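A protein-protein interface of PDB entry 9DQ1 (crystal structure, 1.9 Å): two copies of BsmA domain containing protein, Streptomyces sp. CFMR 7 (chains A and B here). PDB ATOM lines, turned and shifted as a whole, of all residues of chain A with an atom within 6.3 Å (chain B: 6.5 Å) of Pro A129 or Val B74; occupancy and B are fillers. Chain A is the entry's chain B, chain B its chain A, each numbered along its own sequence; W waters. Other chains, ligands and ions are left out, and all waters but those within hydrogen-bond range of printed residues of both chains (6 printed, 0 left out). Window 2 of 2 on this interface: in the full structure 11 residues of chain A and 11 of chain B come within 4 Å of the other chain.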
ATOM      1  N   MET A  33       6.426  20.951 -36.783  1.00  0.00           N
ATOM      2  CA  MET A  33       7.007  19.951 -35.906  1.00  0.00           C
ATOM      3  C   MET A  33       8.360  19.500 -36.417  1.00  0.00           C
ATOM      4  O   MET A  33       8.613  19.484 -37.623  1.00  0.00           O
ATOM      5  CB  MET A  33       6.137  18.716 -35.786  1.00  0.00           C
ATOM      6  CG  MET A  33       6.251  18.122 -34.445  1.00  0.00           C
ATOM      7  SD  MET A  33       4.785  18.724 -33.642  1.00  0.00           S
ATOM      8  CE  MET A  33       3.655  17.652 -34.501  1.00  0.00           C
ATOM      9  N   GLY A  34       9.218  19.099 -35.478  1.00  0.00           N
ATOM     10  CA  GLY A  34      10.503  18.526 -35.809  1.00  0.00           C
ATOM     11  C   GLY A  34      11.614  19.517 -36.079  1.00  0.00           C
ATOM     12  O   GLY A  34      12.747  19.087 -36.340  1.00  0.00           O
ATOM     13  N   ASN A  35      11.328  20.813 -36.036  1.00  0.00           N
ATOM     14  CA  ASN A  35      12.347  21.860 -36.147  1.00  0.00           C
ATOM     15  C   ASN A  35      13.300  21.615 -37.312  1.00  0.00           C
ATOM     16  O   ASN A  35      14.534  21.621 -37.163  1.00  0.00           O
ATOM     17  CB  ASN A  35      13.110  22.004 -34.833  1.00  0.00           C
ATOM     18  CG  ASN A  35      12.274  22.702 -33.782  1.00  0.00           C
ATOM     19  OD1 ASN A  35      12.137  23.924 -33.811  1.00  0.00           O
ATOM     20  ND2 ASN A  35      11.690  21.935 -32.877  1.00  0.00           N
ATOM     21  N   ARG A  38      11.679  17.191 -40.102  1.00  0.00           N
ATOM     22  CA  ARG A  38      10.500  16.451 -40.532  1.00  0.00           C
ATOM     23  C   ARG A  38       9.952  17.005 -41.839  1.00  0.00           C
ATOM     24  O   ARG A  38       9.952  18.221 -42.066  1.00  0.00           O
ATOM     25  CB  ARG A  38       9.391  16.508 -39.478  1.00  0.00           C
ATOM     26  CG  ARG A  38       8.285  15.500 -39.730  1.00  0.00           C
ATOM     27  CD  ARG A  38       7.357  15.421 -38.543  1.00  0.00           C
ATOM     28  NE  ARG A  38       7.991  14.881 -37.348  1.00  0.00           N
ATOM     29  CZ  ARG A  38       7.316  14.555 -36.256  1.00  0.00           C
ATOM     30  NH1 ARG A  38       5.999  14.684 -36.202  1.00  0.00           N
ATOM     31  NH2 ARG A  38       7.978  14.092 -35.193  1.00  0.00           N
ATOM     32  N   ASN A  72      -1.536  16.611 -27.739  1.00  0.00           N
ATOM     33  CA  ASN A  72      -0.274  16.954 -28.386  1.00  0.00           C
ATOM     34  C   ASN A  72       0.159  18.325 -27.877  1.00  0.00           C
ATOM     35  O   ASN A  72      -0.292  19.352 -28.402  1.00  0.00           O
ATOM     36  CB  ASN A  72      -0.431  16.949 -29.899  1.00  0.00           C
ATOM     37  CG  ASN A  72       0.885  17.121 -30.625  1.00  0.00           C
ATOM     38  OD1 ASN A  72       1.830  17.697 -30.087  1.00  0.00           O
ATOM     39  ND2 ASN A  72       0.957  16.609 -31.855  1.00  0.00           N
ATOM     40  N   PRO A  73       1.041  18.387 -26.880  1.00  0.00           N
ATOM     41  CA  PRO A  73       1.378  19.688 -26.286  1.00  0.00           C
ATOM     42  C   PRO A  73       2.260  20.552 -27.162  1.00  0.00           C
ATOM     43  O   PRO A  73       2.359  21.759 -26.911  1.00  0.00           O
ATOM     44  CB  PRO A  73       2.105  19.300 -24.991  1.00  0.00           C
ATOM     45  CG  PRO A  73       2.688  17.967 -25.295  1.00  0.00           C
ATOM     46  CD  PRO A  73       1.678  17.274 -26.166  1.00  0.00           C
ATOM     47  N   VAL A  74       2.902  19.984 -28.177  1.00  0.00           N
ATOM     48  CA  VAL A  74       3.825  20.748 -29.004  1.00  0.00           C
ATOM     49  C   VAL A  74       3.236  21.123 -30.363  1.00  0.00           C
ATOM     50  O   VAL A  74       3.686  22.106 -30.972  1.00  0.00           O
ATOM     51  CB  VAL A  74       5.151  19.976 -29.171  1.00  0.00           C
ATOM     52  CG1 VAL A  74       5.881  19.899 -27.825  1.00  0.00           C
ATOM     53  CG2 VAL A  74       4.913  18.566 -29.760  1.00  0.00           C
ATOM     54  N   PRO A 126      13.683  13.783 -34.049  1.00  0.00           N
ATOM     55  CA  PRO A 126      12.642  13.454 -33.062  1.00  0.00           C
ATOM     56  C   PRO A 126      11.419  12.864 -33.744  1.00  0.00           C
ATOM     57  O   PRO A 126      10.920  13.405 -34.727  1.00  0.00           O
ATOM     58  CB  PRO A 126      12.314  14.804 -32.407  1.00  0.00           C
ATOM     59  CG  PRO A 126      13.391  15.759 -32.866  1.00  0.00           C
ATOM     60  CD  PRO A 126      13.879  15.233 -34.193  1.00  0.00           C
ATOM     61  N   LEU A 127      10.928  11.755 -33.201  1.00  0.00           N
ATOM     62  CA  LEU A 127       9.739  11.099 -33.725  1.00  0.00           C
ATOM     63  C   LEU A 127       8.494  11.409 -32.913  1.00  0.00           C
ATOM     64  O   LEU A 127       7.424  11.599 -33.488  1.00  0.00           O
ATOM     65  CB  LEU A 127       9.958   9.579 -33.771  1.00  0.00           C
ATOM     66  CG  LEU A 127      11.070   9.212 -34.764  1.00  0.00           C
ATOM     67  CD1 LEU A 127      11.372   7.705 -34.725  1.00  0.00           C
ATOM     68  CD2 LEU A 127      10.720   9.679 -36.195  1.00  0.00           C
ATOM     69  N   THR A 128       8.589  11.439 -31.587  1.00  0.00           N
ATOM     70  CA  THR A 128       7.449  11.779 -30.732  1.00  0.00           C
ATOM     71  C   THR A 128       7.880  12.841 -29.729  1.00  0.00           C
ATOM     72  O   THR A 128       8.007  12.572 -28.527  1.00  0.00           O
ATOM     73  CB  THR A 128       6.884  10.548 -30.020  1.00  0.00           C
ATOM     74  OG1 THR A 128       7.899   9.951 -29.204  1.00  0.00           O
ATOM     75  CG2 THR A 128       6.405   9.521 -31.042  1.00  0.00           C
ATOM     76  N   PRO A 129       8.077  14.079 -30.189  1.00  0.00           N
ATOM     77  CA  PRO A 129       8.347  15.166 -29.238  1.00  0.00           C
ATOM     78  C   PRO A 129       7.195  15.413 -28.292  1.00  0.00           C
ATOM     79  O   PRO A 129       7.372  16.118 -27.291  1.00  0.00           O
ATOM     80  CB  PRO A 129       8.615  16.371 -30.148  1.00  0.00           C
ATOM     81  CG  PRO A 129       7.819  16.078 -31.375  1.00  0.00           C
ATOM     82  CD  PRO A 129       7.914  14.574 -31.565  1.00  0.00           C
ATOM     83  N   GLU A 130       6.021  14.839 -28.573  1.00  0.00           N
ATOM     84  CA  GLU A 130       4.917  14.851 -27.623  1.00  0.00           C
ATOM     85  C   GLU A 130       5.257  14.122 -26.330  1.00  0.00           C
ATOM     86  O   GLU A 130       4.545  14.291 -25.331  1.00  0.00           O
ATOM     87  CB  GLU A 130       3.677  14.193 -28.243  1.00  0.00           C
ATOM     88  CG  GLU A 130       3.229  14.781 -29.576  1.00  0.00           C
ATOM     89  CD  GLU A 130       3.959  14.218 -30.778  1.00  0.00           C
ATOM     90  OE1 GLU A 130       5.047  13.608 -30.626  1.00  0.00           O
ATOM     91  OE2 GLU A 130       3.446  14.394 -31.896  1.00  0.00           O
ATOM     92  N   GLY A 131       6.310  13.309 -26.328  1.00  0.00           N
ATOM     93  CA  GLY A 131       6.538  12.399 -25.226  1.00  0.00           C
ATOM     94  C   GLY A 131       5.595  11.210 -25.319  1.00  0.00           C
ATOM     95  O   GLY A 131       4.995  10.934 -26.363  1.00  0.00           O
ATOM     96  N   VAL A 188       8.278   6.999 -29.218  1.00  0.00           N
ATOM     97  CA  VAL A 188       9.339   6.378 -30.004  1.00  0.00           C
ATOM     98  C   VAL A 188      10.619   7.150 -29.723  1.00  0.00           C
ATOM     99  O   VAL A 188      10.603   8.389 -29.678  1.00  0.00           O
ATOM    100  CB  VAL A 188       9.016   6.384 -31.512  1.00  0.00           C
ATOM    101  CG1 VAL A 188      10.036   5.518 -32.268  1.00  0.00           C
ATOM    102  CG2 VAL A 188       7.582   5.889 -31.786  1.00  0.00           C
ATOM    103  N   ASP A 190      14.229   8.842 -30.494  1.00  0.00           N
ATOM    104  CA  ASP A 190      14.726   9.588 -31.644  1.00  0.00           C
ATOM    105  C   ASP A 190      15.431   8.677 -32.640  1.00  0.00           C
ATOM    106  O   ASP A 190      16.114   7.722 -32.266  1.00  0.00           O
ATOM    107  CB  ASP A 190      15.730  10.662 -31.221  1.00  0.00           C
ATOM    108  CG  ASP A 190      15.116  11.773 -30.384  1.00  0.00           C
ATOM    109  OD1 ASP A 190      13.871  11.883 -30.288  1.00  0.00           O
ATOM    110  OD2 ASP A 190      15.917  12.547 -29.814  1.00  0.00           O
ATOM    111  N   TYR B  32      16.616  24.812 -33.466  1.00  0.00           N
ATOM    112  CA  TYR B  32      16.302  23.667 -32.620  1.00  0.00           C
ATOM    113  C   TYR B  32      14.981  23.776 -31.887  1.00  0.00           C
ATOM    114  O   TYR B  32      14.460  22.747 -31.427  1.00  0.00           O
ATOM    115  CB  TYR B  32      17.409  23.469 -31.576  1.00  0.00           C
ATOM    116  CG  TYR B  32      18.786  23.388 -32.186  1.00  0.00           C
ATOM    117  CD1 TYR B  32      19.300  22.176 -32.630  1.00  0.00           C
ATOM    118  CD2 TYR B  32      19.573  24.527 -32.328  1.00  0.00           C
ATOM    119  CE1 TYR B  32      20.577  22.094 -33.188  1.00  0.00           C
ATOM    120  CE2 TYR B  32      20.844  24.456 -32.895  1.00  0.00           C
ATOM    121  CZ  TYR B  32      21.338  23.246 -33.323  1.00  0.00           C
ATOM    122  OH  TYR B  32      22.606  23.201 -33.866  1.00  0.00           O
ATOM    123  N   MET B  33      14.447  24.982 -31.718  1.00  0.00           N
ATOM    124  CA  MET B  33      13.235  25.151 -30.931  1.00  0.00           C
ATOM    125  C   MET B  33      12.352  26.209 -31.557  1.00  0.00           C
ATOM    126  O   MET B  33      12.838  27.159 -32.178  1.00  0.00           O
ATOM    127  CB  MET B  33      13.548  25.520 -29.488  1.00  0.00           C
ATOM    128  CG  MET B  33      14.093  24.331 -28.703  1.00  0.00           C
ATOM    129  SD  MET B  33      14.228  24.671 -26.965  1.00  0.00           S
ATOM    130  CE  MET B  33      12.526  24.627 -26.419  1.00  0.00           C
ATOM    131  N   LYS B  69      17.940  16.327 -21.175  1.00  0.00           N
ATOM    132  CA  LYS B  69      16.589  15.896 -21.522  1.00  0.00           C
ATOM    133  C   LYS B  69      15.684  15.834 -20.295  1.00  0.00           C
ATOM    134  O   LYS B  69      14.473  16.081 -20.399  1.00  0.00           O
ATOM    135  CB  LYS B  69      16.633  14.540 -22.227  1.00  0.00           C
ATOM    136  CG  LYS B  69      16.245  14.640 -23.679  1.00  0.00           C
ATOM    137  CD  LYS B  69      16.293  13.298 -24.365  1.00  0.00           C
ATOM    138  CE  LYS B  69      17.156  13.368 -25.616  1.00  0.00           C
ATOM    139  NZ  LYS B  69      16.774  12.312 -26.597  1.00  0.00           N
ATOM    140  N   ASN B  72      14.577  19.487 -20.163  1.00  0.00           N
ATOM    141  CA  ASN B  72      14.036  20.029 -21.405  1.00  0.00           C
ATOM    142  C   ASN B  72      13.728  18.867 -22.335  1.00  0.00           C
ATOM    143  O   ASN B  72      14.628  18.377 -23.032  1.00  0.00           O
ATOM    144  CB  ASN B  72      15.019  20.991 -22.051  1.00  0.00           C
ATOM    145  CG  ASN B  72      14.415  21.739 -23.227  1.00  0.00           C
ATOM    146  OD1 ASN B  72      13.519  21.243 -23.911  1.00  0.00           O
ATOM    147  ND2 ASN B  72      14.898  22.946 -23.456  1.00  0.00           N
ATOM    148  N   PRO B  73      12.470  18.428 -22.407  1.00  0.00           N
ATOM    149  CA  PRO B  73      12.146  17.251 -23.216  1.00  0.00           C
ATOM    150  C   PRO B  73      12.257  17.487 -24.709  1.00  0.00           C
ATOM    151  O   PRO B  73      12.394  16.514 -25.454  1.00  0.00           O
ATOM    152  CB  PRO B  73      10.694  16.939 -22.809  1.00  0.00           C
ATOM    153  CG  PRO B  73      10.147  18.257 -22.365  1.00  0.00           C
ATOM    154  CD  PRO B  73      11.298  18.962 -21.700  1.00  0.00           C
ATOM    155  N   VAL B  74      12.194  18.736 -25.173  1.00  0.00           N
ATOM    156  CA  VAL B  74      12.170  19.007 -26.603  1.00  0.00           C
ATOM    157  C   VAL B  74      13.494  19.552 -27.147  1.00  0.00           C
ATOM    158  O   VAL B  74      13.739  19.460 -28.362  1.00  0.00           O
ATOM    159  CB  VAL B  74      10.997  19.956 -26.945  1.00  0.00           C
ATOM    160  CG1 VAL B  74       9.648  19.232 -26.737  1.00  0.00           C
ATOM    161  CG2 VAL B  74      11.037  21.237 -26.122  1.00  0.00           C
ATOM    162  N   GLY B  75      14.358  20.088 -26.298  1.00  0.00           N
ATOM    163  CA  GLY B  75      15.604  20.642 -26.783  1.00  0.00           C
ATOM    164  C   GLY B  75      16.801  20.224 -25.960  1.00  0.00           C
ATOM    165  O   GLY B  75      17.854  20.864 -26.029  1.00  0.00           O
ATOM    166  N   GLY B  76      16.648  19.148 -25.181  1.00  0.00           N
ATOM    167  CA  GLY B  76      17.706  18.644 -24.335  1.00  0.00           C
ATOM    168  C   GLY B  76      18.446  17.472 -24.962  1.00  0.00           C
ATOM    169  O   GLY B  76      17.961  16.815 -25.887  1.00  0.00           O
ATOM    170  N   ILE B  78      21.192  17.433 -26.763  1.00  0.00           N
ATOM    171  CA  ILE B  78      21.813  17.663 -28.061  1.00  0.00           C
ATOM    172  C   ILE B  78      22.650  18.942 -28.017  1.00  0.00           C
ATOM    173  O   ILE B  78      22.398  19.858 -27.221  1.00  0.00           O
ATOM    174  CB  ILE B  78      20.771  17.756 -29.197  1.00  0.00           C
ATOM    175  CG1 ILE B  78      19.769  18.862 -28.889  1.00  0.00           C
ATOM    176  CG2 ILE B  78      20.031  16.407 -29.410  1.00  0.00           C
ATOM    177  CD1 ILE B  78      18.988  19.318 -30.112  1.00  0.00           C
ATOM    178  N   ARG B  80      23.452  22.400 -29.367  1.00  0.00           N
ATOM    179  CA  ARG B  80      22.699  23.442 -30.037  1.00  0.00           C
ATOM    180  C   ARG B  80      23.673  24.560 -30.389  1.00  0.00           C
ATOM    181  O   ARG B  80      24.176  25.264 -29.504  1.00  0.00           O
ATOM    182  CB  ARG B  80      21.526  23.893 -29.158  1.00  0.00           C
ATOM    183  CG  ARG B  80      20.518  22.729 -28.971  1.00  0.00           C
ATOM    184  CD  ARG B  80      19.492  22.938 -27.846  1.00  0.00           C
ATOM    185  NE  ARG B  80      18.814  24.231 -27.905  1.00  0.00           N
ATOM    186  CZ  ARG B  80      17.981  24.668 -26.968  1.00  0.00           C
ATOM    187  NH1 ARG B  80      17.640  23.903 -25.942  1.00  0.00           N
ATOM    188  NH2 ARG B  80      17.494  25.908 -27.053  1.00  0.00           N
ATOM    189  N   THR B 128       7.296  28.301 -23.923  1.00  0.00           N
ATOM    190  CA  THR B 128       7.806  27.175 -23.144  1.00  0.00           C
ATOM    191  C   THR B 128       7.226  25.870 -23.691  1.00  0.00           C
ATOM    192  O   THR B 128       6.412  25.221 -23.035  1.00  0.00           O
ATOM    193  CB  THR B 128       7.487  27.354 -21.652  1.00  0.00           C
ATOM    194  OG1 THR B 128       6.076  27.467 -21.469  1.00  0.00           O
ATOM    195  CG2 THR B 128       8.119  28.643 -21.127  1.00  0.00           C
ATOM    196  N   PRO B 129       7.664  25.433 -24.877  1.00  0.00           N
ATOM    197  CA  PRO B 129       7.213  24.125 -25.387  1.00  0.00           C
ATOM    198  C   PRO B 129       7.625  22.975 -24.490  1.00  0.00           C
ATOM    199  O   PRO B 129       7.086  21.868 -24.640  1.00  0.00           O
ATOM    200  CB  PRO B 129       7.882  24.031 -26.766  1.00  0.00           C
ATOM    201  CG  PRO B 129       9.074  24.921 -26.658  1.00  0.00           C
ATOM    202  CD  PRO B 129       8.639  26.063 -25.782  1.00  0.00           C
ATOM    203  N   GLU B 130       8.574  23.204 -23.579  1.00  0.00           N
ATOM    204  CA  GLU B 130       8.875  22.241 -22.528  1.00  0.00           C
ATOM    205  C   GLU B 130       7.672  21.939 -21.645  1.00  0.00           C
ATOM    206  O   GLU B 130       7.692  20.936 -20.915  1.00  0.00           O
ATOM    207  CB  GLU B 130      10.012  22.764 -21.645  1.00  0.00           C
ATOM    208  CG  GLU B 130      11.274  23.182 -22.399  1.00  0.00           C
ATOM    209  CD  GLU B 130      11.244  24.620 -22.906  1.00  0.00           C
ATOM    210  OE1 GLU B 130      10.152  25.233 -23.007  1.00  0.00           O
ATOM    211  OE2 GLU B 130      12.327  25.144 -23.227  1.00  0.00           O
ATOM    212  N   GLY B 131       6.637  22.784 -21.669  1.00  0.00           N
ATOM    213  CA  GLY B 131       5.591  22.654 -20.665  1.00  0.00           C
ATOM    214  C   GLY B 131       6.078  23.228 -19.337  1.00  0.00           C
ATOM    215  O   GLY B 131       7.037  24.004 -19.282  1.00  0.00           O
HETATM  216  O   HOH W   1       9.539  15.161 -25.826  1.00  0.00           O
HETATM  217  O   HOH W   2      14.975   9.610 -27.596  1.00  0.00           O
HETATM  218  O   HOH W   3      13.038  25.981 -35.345  1.00  0.00           O
HETATM  219  O   HOH W   4      12.458  21.314 -30.190  1.00  0.00           O
HETATM  220  O   HOH W   5      18.208  12.471 -28.692  1.00  0.00           O
HETATM  221  O   HOH W   6       4.257  22.317 -24.878  1.00  0.00           O
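Val A74 touches its own counterpart, Val B74. Val A74 touches Pro B129, and with the chains exchanged Pro A129 touches Val B74.
Water W5 lies within hydrogen-bond range of the side-chain amino group (NZ) of Lys B69 (2.5 Å) and the side-chain carboxylate (OD2) of Asp A190 (2.6 Å). Water W3 bridges OD1 of Asn A35 (2.7 Å) and O of Met B33 (3.4 Å). Water W4 lies within hydrogen-bond range of O of Tyr B32 (2.8 Å), ND2 of Asn A35 (2.9 Å) and O of Val B74 (2.9 Å). Water W1 bridges O of Pro A129 (2.8 Å) and O of Pro B73 (3.2 Å). Water W6 lies within hydrogen-bond range of the backbone carbonyl oxygen (O) of Pro A73 (2.8 Å) and the backbone carbonyl oxygen (O) of Pro B129 (2.9 Å). Water W2 lies within hydrogen-bond range of the backbone NH (N) of Asp A190 and the side-chain amino group (NZ) of Lys B69.
The side-chain amide oxygen of Asn A35 lies close to the backbone NH of Met B33, at 3.3 Å. The side-chain carboxylate of Asp A190 lies within salt-bridge range of the side-chain amino group of Lys B69. The backbone carbonyl oxygen of Tyr B32 lies close to the side-chain amide nitrogen of Asn A35 (3.2 Å).
The backbone NH (N) of Val A74 lies within hydrogen-bond range of the side-chain amide oxygen (OD1) of Asn A72 (3.2 Å). N of Val B74 sits at hydrogen-bond distance from OD1 of Asn B72, 3.1 Å away. NH2 of Arg B80 is in hydrogen-bond range of SD of Met B33 (3.5 Å).
Of the 14 printed residues of chain B, 5 touch a printed residue of chain A. Printed residues of chain A that touch a printed residue of chain B: Asn A35, Val A74, Pro A129 and Asp A190.
Among the printed residues, pairs that only touch across the chains: Pro A129 with Val B74 (3.9 Å), Val A74 with Pro B129 (3.9 Å) and Val A74 with Val B74 (3.98 Å).
Printed residues of chain B within 4 Å of Val A74: Val B74 and Pro B129. Of chain B, only Val B74 (3.9 Å) comes within 4 Å of Pro A129. Of the printed residues of chain A, Tyr B32 touches Asn A35 (3.2 Å). Of the printed residues of chain A, Lys B69 touches Asp A190. Of chain A, only Val A74 (3.98 Å) and Pro A129 (3.9 Å) come within 4 Å of Val B74. The nearest residue of chain A that does not touch Val B74 is Asn A35 (5.5 Å). The nearest printed residue of chain B that does not touch Asn A35 is Val B74 (5.5 Å).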
